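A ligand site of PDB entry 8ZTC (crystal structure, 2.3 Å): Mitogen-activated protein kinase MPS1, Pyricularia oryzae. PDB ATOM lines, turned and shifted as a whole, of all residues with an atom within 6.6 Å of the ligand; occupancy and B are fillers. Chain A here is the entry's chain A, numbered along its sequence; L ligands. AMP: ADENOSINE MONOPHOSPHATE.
N of Glu 115 lies within hydrogen-bond range of O of Ala 61, at 2.9 Å. The backbone NH (N) of Leu 40 lies within hydrogen-bond range of the backbone carbonyl oxygen (O) of Val 48, at 3.0 Å. The backbone carbonyl oxygen (O) of Gly 41 lies within hydrogen-bond range of the backbone NH (N) of Val 48, at 3.2 Å.
The backbone carbonyl oxygen (O) of Glu 116 lies within hydrogen-bond range of a nitrogen (N6) of the ligand. The backbone NH of Met 118 lies within hydrogen-bond range of a nitrogen (N1) of the ligand (3.1 Å). The backbone carbonyl oxygen (O) of Leu 40 is in hydrogen-bond range of an oxygen (O3') of the ligand (3.3 Å). A nitrogen (N6) of the ligand lies within hydrogen-bond range of the side-chain carboxylate (OE1) of Glu 115, at 3.4 Å.
Merely in contact with the ligand: Asp 121 (3.5 Å), Leu 167 (3.6 Å), Val 48 (3.6 Å), Ala 61 (3.8 Å) and Leu 117 (3.9 Å). Hydrophobic or aromatic side chains that line the ligand: Leu 40, Val 48, Ala 61, Leu 117, Met 118 and Leu 167. Along chain A the residues within 4 Å of the ligand span positions 40 to 167.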
ATOM      1  N   LEU A  40       2.555  10.544  -1.944  1.00  0.00           N
ATOM      2  CA  LEU A  40       1.161  10.696  -2.352  1.00  0.00           C
ATOM      3  C   LEU A  40       0.963  11.175  -3.773  1.00  0.00           C
ATOM      4  O   LEU A  40      -0.151  11.067  -4.288  1.00  0.00           O
ATOM      5  CB  LEU A  40       0.421  11.648  -1.399  1.00  0.00           C
ATOM      6  CG  LEU A  40       0.162  11.083   0.007  1.00  0.00           C
ATOM      7  CD1 LEU A  40      -0.758  11.986   0.799  1.00  0.00           C
ATOM      8  CD2 LEU A  40      -0.421   9.679  -0.093  1.00  0.00           C
ATOM      9  N   GLY A  41       1.997  11.684  -4.437  1.00  0.00           N
ATOM     10  CA  GLY A  41       1.876  12.001  -5.838  1.00  0.00           C
ATOM     11  C   GLY A  41       2.687  13.220  -6.209  1.00  0.00           C
ATOM     12  O   GLY A  41       3.269  13.904  -5.378  1.00  0.00           O
ATOM     13  N   GLN A  42       2.712  13.488  -7.521  1.00  0.00           N
ATOM     14  CA  GLN A  42       3.393  14.626  -8.097  1.00  0.00           C
ATOM     15  C   GLN A  42       2.415  15.470  -8.910  1.00  0.00           C
ATOM     16  O   GLN A  42       1.269  15.086  -9.145  1.00  0.00           O
ATOM     17  CB  GLN A  42       4.553  14.191  -9.004  1.00  0.00           C
ATOM     18  CG  GLN A  42       5.913  14.253  -8.345  1.00  0.00           C
ATOM     19  CD  GLN A  42       7.010  14.670  -9.305  1.00  0.00           C
ATOM     20  OE1 GLN A  42       6.763  14.917 -10.480  1.00  0.00           O
ATOM     21  NE2 GLN A  42       8.238  14.763  -8.794  1.00  0.00           N
ATOM     22  N   GLY A  43       2.907  16.635  -9.329  1.00  0.00           N
ATOM     23  CA  GLY A  43       2.189  17.512 -10.228  1.00  0.00           C
ATOM     24  C   GLY A  43       3.198  18.438 -10.873  1.00  0.00           C
ATOM     25  O   GLY A  43       4.399  18.375 -10.592  1.00  0.00           O
ATOM     26  N   ALA A  44       2.702  19.314 -11.740  1.00  0.00           N
ATOM     27  CA  ALA A  44       3.577  20.324 -12.322  1.00  0.00           C
ATOM     28  C   ALA A  44       3.944  21.404 -11.331  1.00  0.00           C
ATOM     29  O   ALA A  44       4.778  22.266 -11.652  1.00  0.00           O
ATOM     30  CB  ALA A  44       2.913  20.951 -13.554  1.00  0.00           C
ATOM     31  N   TYR A  45       3.363  21.393 -10.126  1.00  0.00           N
ATOM     32  CA  TYR A  45       3.532  22.474  -9.175  1.00  0.00           C
ATOM     33  C   TYR A  45       4.105  22.034  -7.833  1.00  0.00           C
ATOM     34  O   TYR A  45       4.408  22.905  -7.004  1.00  0.00           O
ATOM     35  CB  TYR A  45       2.199  23.207  -8.953  1.00  0.00           C
ATOM     36  CG  TYR A  45       1.518  23.579 -10.242  1.00  0.00           C
ATOM     37  CD1 TYR A  45       2.230  24.203 -11.264  1.00  0.00           C
ATOM     38  CD2 TYR A  45       0.171  23.294 -10.463  1.00  0.00           C
ATOM     39  CE1 TYR A  45       1.622  24.543 -12.453  1.00  0.00           C
ATOM     40  CE2 TYR A  45      -0.437  23.635 -11.652  1.00  0.00           C
ATOM     41  CZ  TYR A  45       0.288  24.259 -12.647  1.00  0.00           C
ATOM     42  OH  TYR A  45      -0.321  24.600 -13.837  1.00  0.00           O
ATOM     43  N   GLY A  46       4.257  20.742  -7.595  1.00  0.00           N
ATOM     44  CA  GLY A  46       4.897  20.299  -6.376  1.00  0.00           C
ATOM     45  C   GLY A  46       4.638  18.828  -6.102  1.00  0.00           C
ATOM     46  O   GLY A  46       4.048  18.119  -6.918  1.00  0.00           O
ATOM     47  N   ILE A  47       5.103  18.399  -4.927  1.00  0.00           N
ATOM     48  CA  ILE A  47       4.994  17.020  -4.478  1.00  0.00           C
ATOM     49  C   ILE A  47       4.269  17.007  -3.137  1.00  0.00           C
ATOM     50  O   ILE A  47       4.273  17.981  -2.391  1.00  0.00           O
ATOM     51  CB  ILE A  47       6.375  16.342  -4.367  1.00  0.00           C
ATOM     52  CG1 ILE A  47       7.284  17.151  -3.450  1.00  0.00           C
ATOM     53  CG2 ILE A  47       7.031  16.263  -5.730  1.00  0.00           C
ATOM     54  CD1 ILE A  47       8.541  16.405  -3.051  1.00  0.00           C
ATOM     55  N   VAL A  48       3.637  15.868  -2.839  1.00  0.00           N
ATOM     56  CA  VAL A  48       2.794  15.728  -1.655  1.00  0.00           C
ATOM     57  C   VAL A  48       3.152  14.428  -0.934  1.00  0.00           C
ATOM     58  O   VAL A  48       3.285  13.386  -1.567  1.00  0.00           O
ATOM     59  CB  VAL A  48       1.296  15.748  -2.013  1.00  0.00           C
ATOM     60  CG1 VAL A  48       0.439  15.568  -0.765  1.00  0.00           C
ATOM     61  CG2 VAL A  48       0.925  17.028  -2.734  1.00  0.00           C
ATOM     62  N   CYS A  49       3.293  14.514   0.393  1.00  0.00           N
ATOM     63  CA  CYS A  49       3.541  13.350   1.231  1.00  0.00           C
ATOM     64  C   CYS A  49       2.608  13.379   2.439  1.00  0.00           C
ATOM     65  O   CYS A  49       2.081  14.435   2.809  1.00  0.00           O
ATOM     66  CB  CYS A  49       4.995  13.286   1.725  1.00  0.00           C
ATOM     67  SG  CYS A  49       6.251  13.281   0.427  1.00  0.00           S
ATOM     68  N   ALA A  50       2.410  12.214   3.040  1.00  0.00           N
ATOM     69  CA  ALA A  50       1.695  12.094   4.298  1.00  0.00           C
ATOM     70  C   ALA A  50       2.700  11.938   5.432  1.00  0.00           C
ATOM     71  O   ALA A  50       3.827  11.480   5.247  1.00  0.00           O
ATOM     72  CB  ALA A  50       0.731  10.912   4.275  1.00  0.00           C
ATOM     73  N   ALA A  61      -0.999  16.103   5.971  1.00  0.00           N
ATOM     74  CA  ALA A  61      -0.391  16.083   4.657  1.00  0.00           C
ATOM     75  C   ALA A  61       0.534  17.282   4.497  1.00  0.00           C
ATOM     76  O   ALA A  61       0.208  18.380   4.952  1.00  0.00           O
ATOM     77  CB  ALA A  61      -1.458  16.085   3.559  1.00  0.00           C
ATOM     78  N   LYS A  63       2.616  19.475   1.650  1.00  0.00           N
ATOM     79  CA  LYS A  63       2.761  19.783   0.232  1.00  0.00           C
ATOM     80  C   LYS A  63       3.938  20.740   0.035  1.00  0.00           C
ATOM     81  O   LYS A  63       4.018  21.783   0.697  1.00  0.00           O
ATOM     82  CB  LYS A  63       1.477  20.408  -0.308  1.00  0.00           C
ATOM     83  CG  LYS A  63       1.573  20.947  -1.739  1.00  0.00           C
ATOM     84  CD  LYS A  63       0.272  20.699  -2.502  1.00  0.00           C
ATOM     85  CE  LYS A  63      -0.303  21.976  -3.099  1.00  0.00           C
ATOM     86  NZ  LYS A  63       0.282  22.315  -4.428  1.00  0.00           N
ATOM     87  N   THR A  95     -10.517  22.093   2.130  1.00  0.00           N
ATOM     88  CA  THR A  95      -9.291  21.615   2.753  1.00  0.00           C
ATOM     89  C   THR A  95      -8.724  22.676   3.697  1.00  0.00           C
ATOM     90  O   THR A  95      -8.687  23.863   3.372  1.00  0.00           O
ATOM     91  CB  THR A  95      -8.282  21.219   1.663  1.00  0.00           C
ATOM     92  OG1 THR A  95      -7.153  20.567   2.256  1.00  0.00           O
ATOM     93  CG2 THR A  95      -7.816  22.428   0.845  1.00  0.00           C
ATOM     94  N   GLU A 115      -1.424  20.565   5.878  1.00  0.00           N
ATOM     95  CA  GLU A 115      -2.864  20.512   5.683  1.00  0.00           C
ATOM     96  C   GLU A 115      -3.482  19.304   6.371  1.00  0.00           C
ATOM     97  O   GLU A 115      -2.796  18.340   6.727  1.00  0.00           O
ATOM     98  CB  GLU A 115      -3.241  20.432   4.194  1.00  0.00           C
ATOM     99  CG  GLU A 115      -2.670  21.521   3.320  1.00  0.00           C
ATOM    100  CD  GLU A 115      -3.007  21.304   1.850  1.00  0.00           C
ATOM    101  OE1 GLU A 115      -3.594  20.248   1.523  1.00  0.00           O
ATOM    102  OE2 GLU A 115      -2.697  22.206   1.035  1.00  0.00           O
ATOM    103  N   GLU A 116      -4.797  19.364   6.520  1.00  0.00           N
ATOM    104  CA  GLU A 116      -5.574  18.230   6.999  1.00  0.00           C
ATOM    105  C   GLU A 116      -5.483  17.057   6.015  1.00  0.00           C
ATOM    106  O   GLU A 116      -5.523  17.254   4.791  1.00  0.00           O
ATOM    107  CB  GLU A 116      -7.020  18.667   7.224  1.00  0.00           C
ATOM    108  CG  GLU A 116      -8.092  17.642   6.954  1.00  0.00           C
ATOM    109  CD  GLU A 116      -9.485  18.254   7.076  1.00  0.00           C
ATOM    110  OE1 GLU A 116      -9.739  19.275   6.414  1.00  0.00           O
ATOM    111  OE2 GLU A 116     -10.304  17.714   7.854  1.00  0.00           O
ATOM    112  N   LEU A 117      -5.352  15.853   6.547  1.00  0.00           N
ATOM    113  CA  LEU A 117      -5.014  14.667   5.758  1.00  0.00           C
ATOM    114  C   LEU A 117      -6.275  13.913   5.318  1.00  0.00           C
ATOM    115  O   LEU A 117      -7.154  13.639   6.131  1.00  0.00           O
ATOM    116  CB  LEU A 117      -4.109  13.730   6.562  1.00  0.00           C
ATOM    117  CG  LEU A 117      -3.707  12.396   5.918  1.00  0.00           C
ATOM    118  CD1 LEU A 117      -2.939  12.633   4.636  1.00  0.00           C
ATOM    119  CD2 LEU A 117      -2.890  11.562   6.892  1.00  0.00           C
ATOM    120  N   MET A 118      -6.344  13.583   4.032  1.00  0.00           N
ATOM    121  CA  MET A 118      -7.409  12.793   3.444  1.00  0.00           C
ATOM    122  C   MET A 118      -6.835  11.510   2.847  1.00  0.00           C
ATOM    123  O   MET A 118      -5.625  11.298   2.812  1.00  0.00           O
ATOM    124  CB  MET A 118      -8.168  13.586   2.361  1.00  0.00           C
ATOM    125  CG  MET A 118      -8.733  14.947   2.817  1.00  0.00           C
ATOM    126  SD  MET A 118      -9.921  14.884   4.177  1.00  0.00           S
ATOM    127  CE  MET A 118     -11.439  14.460   3.324  1.00  0.00           C
ATOM    128  N   GLU A 119      -7.724  10.640   2.339  1.00  0.00           N
ATOM    129  CA  GLU A 119      -7.311   9.313   1.879  1.00  0.00           C
ATOM    130  C   GLU A 119      -7.149   9.206   0.365  1.00  0.00           C
ATOM    131  O   GLU A 119      -6.117   8.699  -0.091  1.00  0.00           O
ATOM    132  CB  GLU A 119      -8.306   8.268   2.388  1.00  0.00           C
ATOM    133  CG  GLU A 119      -8.654   8.509   3.844  1.00  0.00           C
ATOM    134  CD  GLU A 119      -8.991   7.234   4.586  1.00  0.00           C
ATOM    135  OE1 GLU A 119      -8.321   6.206   4.348  1.00  0.00           O
ATOM    136  OE2 GLU A 119      -9.920   7.276   5.422  1.00  0.00           O
ATOM    137  N   CYS A 120      -8.132   9.641  -0.429  1.00  0.00           N
ATOM    138  CA  CYS A 120      -7.994   9.674  -1.874  1.00  0.00           C
ATOM    139  C   CYS A 120      -8.899  10.764  -2.426  1.00  0.00           C
ATOM    140  O   CYS A 120      -9.614  11.445  -1.684  1.00  0.00           O
ATOM    141  CB  CYS A 120      -8.347   8.331  -2.522  1.00  0.00           C
ATOM    142  SG  CYS A 120      -9.944   7.649  -2.056  1.00  0.00           S
ATOM    143  N   ASP A 121      -8.874  10.926  -3.749  1.00  0.00           N
ATOM    144  CA  ASP A 121      -9.762  11.866  -4.427  1.00  0.00           C
ATOM    145  C   ASP A 121     -10.922  11.122  -5.104  1.00  0.00           C
ATOM    146  O   ASP A 121     -10.921   9.894  -5.217  1.00  0.00           O
ATOM    147  CB  ASP A 121      -8.982  12.708  -5.443  1.00  0.00           C
ATOM    148  CG  ASP A 121      -8.301  11.862  -6.509  1.00  0.00           C
ATOM    149  OD1 ASP A 121      -8.879  10.843  -6.924  1.00  0.00           O
ATOM    150  OD2 ASP A 121      -7.187  12.231  -6.932  1.00  0.00           O
ATOM    151  N   GLY A 164     -10.881  15.177  -9.745  1.00  0.00           N
ATOM    152  CA  GLY A 164      -9.518  15.161  -9.241  1.00  0.00           C
ATOM    153  C   GLY A 164      -9.221  16.203  -8.174  1.00  0.00           C
ATOM    154  O   GLY A 164      -8.251  16.037  -7.428  1.00  0.00           O
ATOM    155  N   ASN A 165     -10.035  17.255  -8.082  1.00  0.00           N
ATOM    156  CA  ASN A 165      -9.839  18.285  -7.063  1.00  0.00           C
ATOM    157  C   ASN A 165     -10.831  18.147  -5.910  1.00  0.00           C
ATOM    158  O   ASN A 165     -11.164  19.142  -5.257  1.00  0.00           O
ATOM    159  CB  ASN A 165      -9.929  19.671  -7.694  1.00  0.00           C
ATOM    160  CG  ASN A 165      -8.759  19.984  -8.627  1.00  0.00           C
ATOM    161  OD1 ASN A 165      -7.703  19.347  -8.535  1.00  0.00           O
ATOM    162  ND2 ASN A 165      -8.935  20.961  -9.504  1.00  0.00           N
ATOM    163  N   LEU A 167     -11.300  15.841  -2.452  1.00  0.00           N
ATOM    164  CA  LEU A 167     -10.702  14.856  -1.549  1.00  0.00           C
ATOM    165  C   LEU A 167     -11.771  14.189  -0.691  1.00  0.00           C
ATOM    166  O   LEU A 167     -12.750  14.818  -0.287  1.00  0.00           O
ATOM    167  CB  LEU A 167      -9.659  15.523  -0.652  1.00  0.00           C
ATOM    168  CG  LEU A 167      -8.528  16.265  -1.366  1.00  0.00           C
ATOM    169  CD1 LEU A 167      -7.563  16.894  -0.357  1.00  0.00           C
ATOM    170  CD2 LEU A 167      -7.785  15.341  -2.314  1.00  0.00           C
ATOM    171  N   CYS A 177     -10.451  21.359  -3.033  1.00  0.00           N
ATOM    172  CA  CYS A 177      -9.053  21.791  -2.921  1.00  0.00           C
ATOM    173  C   CYS A 177      -8.611  22.447  -4.232  1.00  0.00           C
ATOM    174  O   CYS A 177      -9.389  22.560  -5.190  1.00  0.00           O
ATOM    175  CB  CYS A 177      -8.151  20.612  -2.543  1.00  0.00           C
ATOM    176  SG  CYS A 177      -7.785  19.460  -3.887  1.00  0.00           S
ATOM    177  N   ASP A 178      -7.354  22.893  -4.244  1.00  0.00           N
ATOM    178  CA  ASP A 178      -6.662  23.472  -5.400  1.00  0.00           C
ATOM    179  C   ASP A 178      -7.239  24.808  -5.853  1.00  0.00           C
ATOM    180  O   ASP A 178      -8.143  24.850  -6.698  1.00  0.00           O
ATOM    181  CB  ASP A 178      -6.647  22.493  -6.577  1.00  0.00           C
ATOM    182  CG  ASP A 178      -5.547  22.812  -7.591  1.00  0.00           C
ATOM    183  OD1 ASP A 178      -5.065  23.967  -7.617  1.00  0.00           O
ATOM    184  OD2 ASP A 178      -5.164  21.898  -8.342  1.00  0.00           O
HETATM  185  P   AMP L   1      -1.611  17.825  -6.704  1.00  0.00           P
HETATM  186  O1P AMP L   1      -1.869  17.786  -8.187  1.00  0.00           O
HETATM  187  O2P AMP L   1      -2.574  18.677  -5.897  1.00  0.00           O
HETATM  188  O3P AMP L   1      -0.161  18.030  -6.330  1.00  0.00           O
HETATM  189  O5' AMP L   1      -1.911  16.325  -6.229  1.00  0.00           O
HETATM  190  C5' AMP L   1      -0.919  15.542  -5.582  1.00  0.00           C
HETATM  191  C4' AMP L   1      -1.473  14.236  -5.049  1.00  0.00           C
HETATM  192  O4' AMP L   1      -1.653  14.346  -3.615  1.00  0.00           O
HETATM  193  C3' AMP L   1      -2.828  13.819  -5.625  1.00  0.00           C
HETATM  194  O3' AMP L   1      -2.888  12.392  -5.693  1.00  0.00           O
HETATM  195  C2' AMP L   1      -3.804  14.320  -4.567  1.00  0.00           C
HETATM  196  O2' AMP L   1      -5.044  13.632  -4.538  1.00  0.00           O
HETATM  197  C1' AMP L   1      -3.009  14.111  -3.274  1.00  0.00           C
HETATM  198  N9  AMP L   1      -3.369  15.034  -2.200  1.00  0.00           N
HETATM  199  C8  AMP L   1      -3.374  16.377  -2.308  1.00  0.00           C
HETATM  200  N7  AMP L   1      -3.740  16.964  -1.143  1.00  0.00           N
HETATM  201  C5  AMP L   1      -3.987  15.979  -0.256  1.00  0.00           C
HETATM  202  C6  AMP L   1      -4.423  15.918   1.151  1.00  0.00           C
HETATM  203  N6  AMP L   1      -4.669  17.055   1.855  1.00  0.00           N
HETATM  204  N1  AMP L   1      -4.565  14.699   1.716  1.00  0.00           N
HETATM  205  C2  AMP L   1      -4.311  13.566   1.022  1.00  0.00           C
HETATM  206  N3  AMP L   1      -3.917  13.551  -0.276  1.00  0.00           N
HETATM  207  C4  AMP L   1      -3.740  14.710  -0.952  1.00  0.00           C
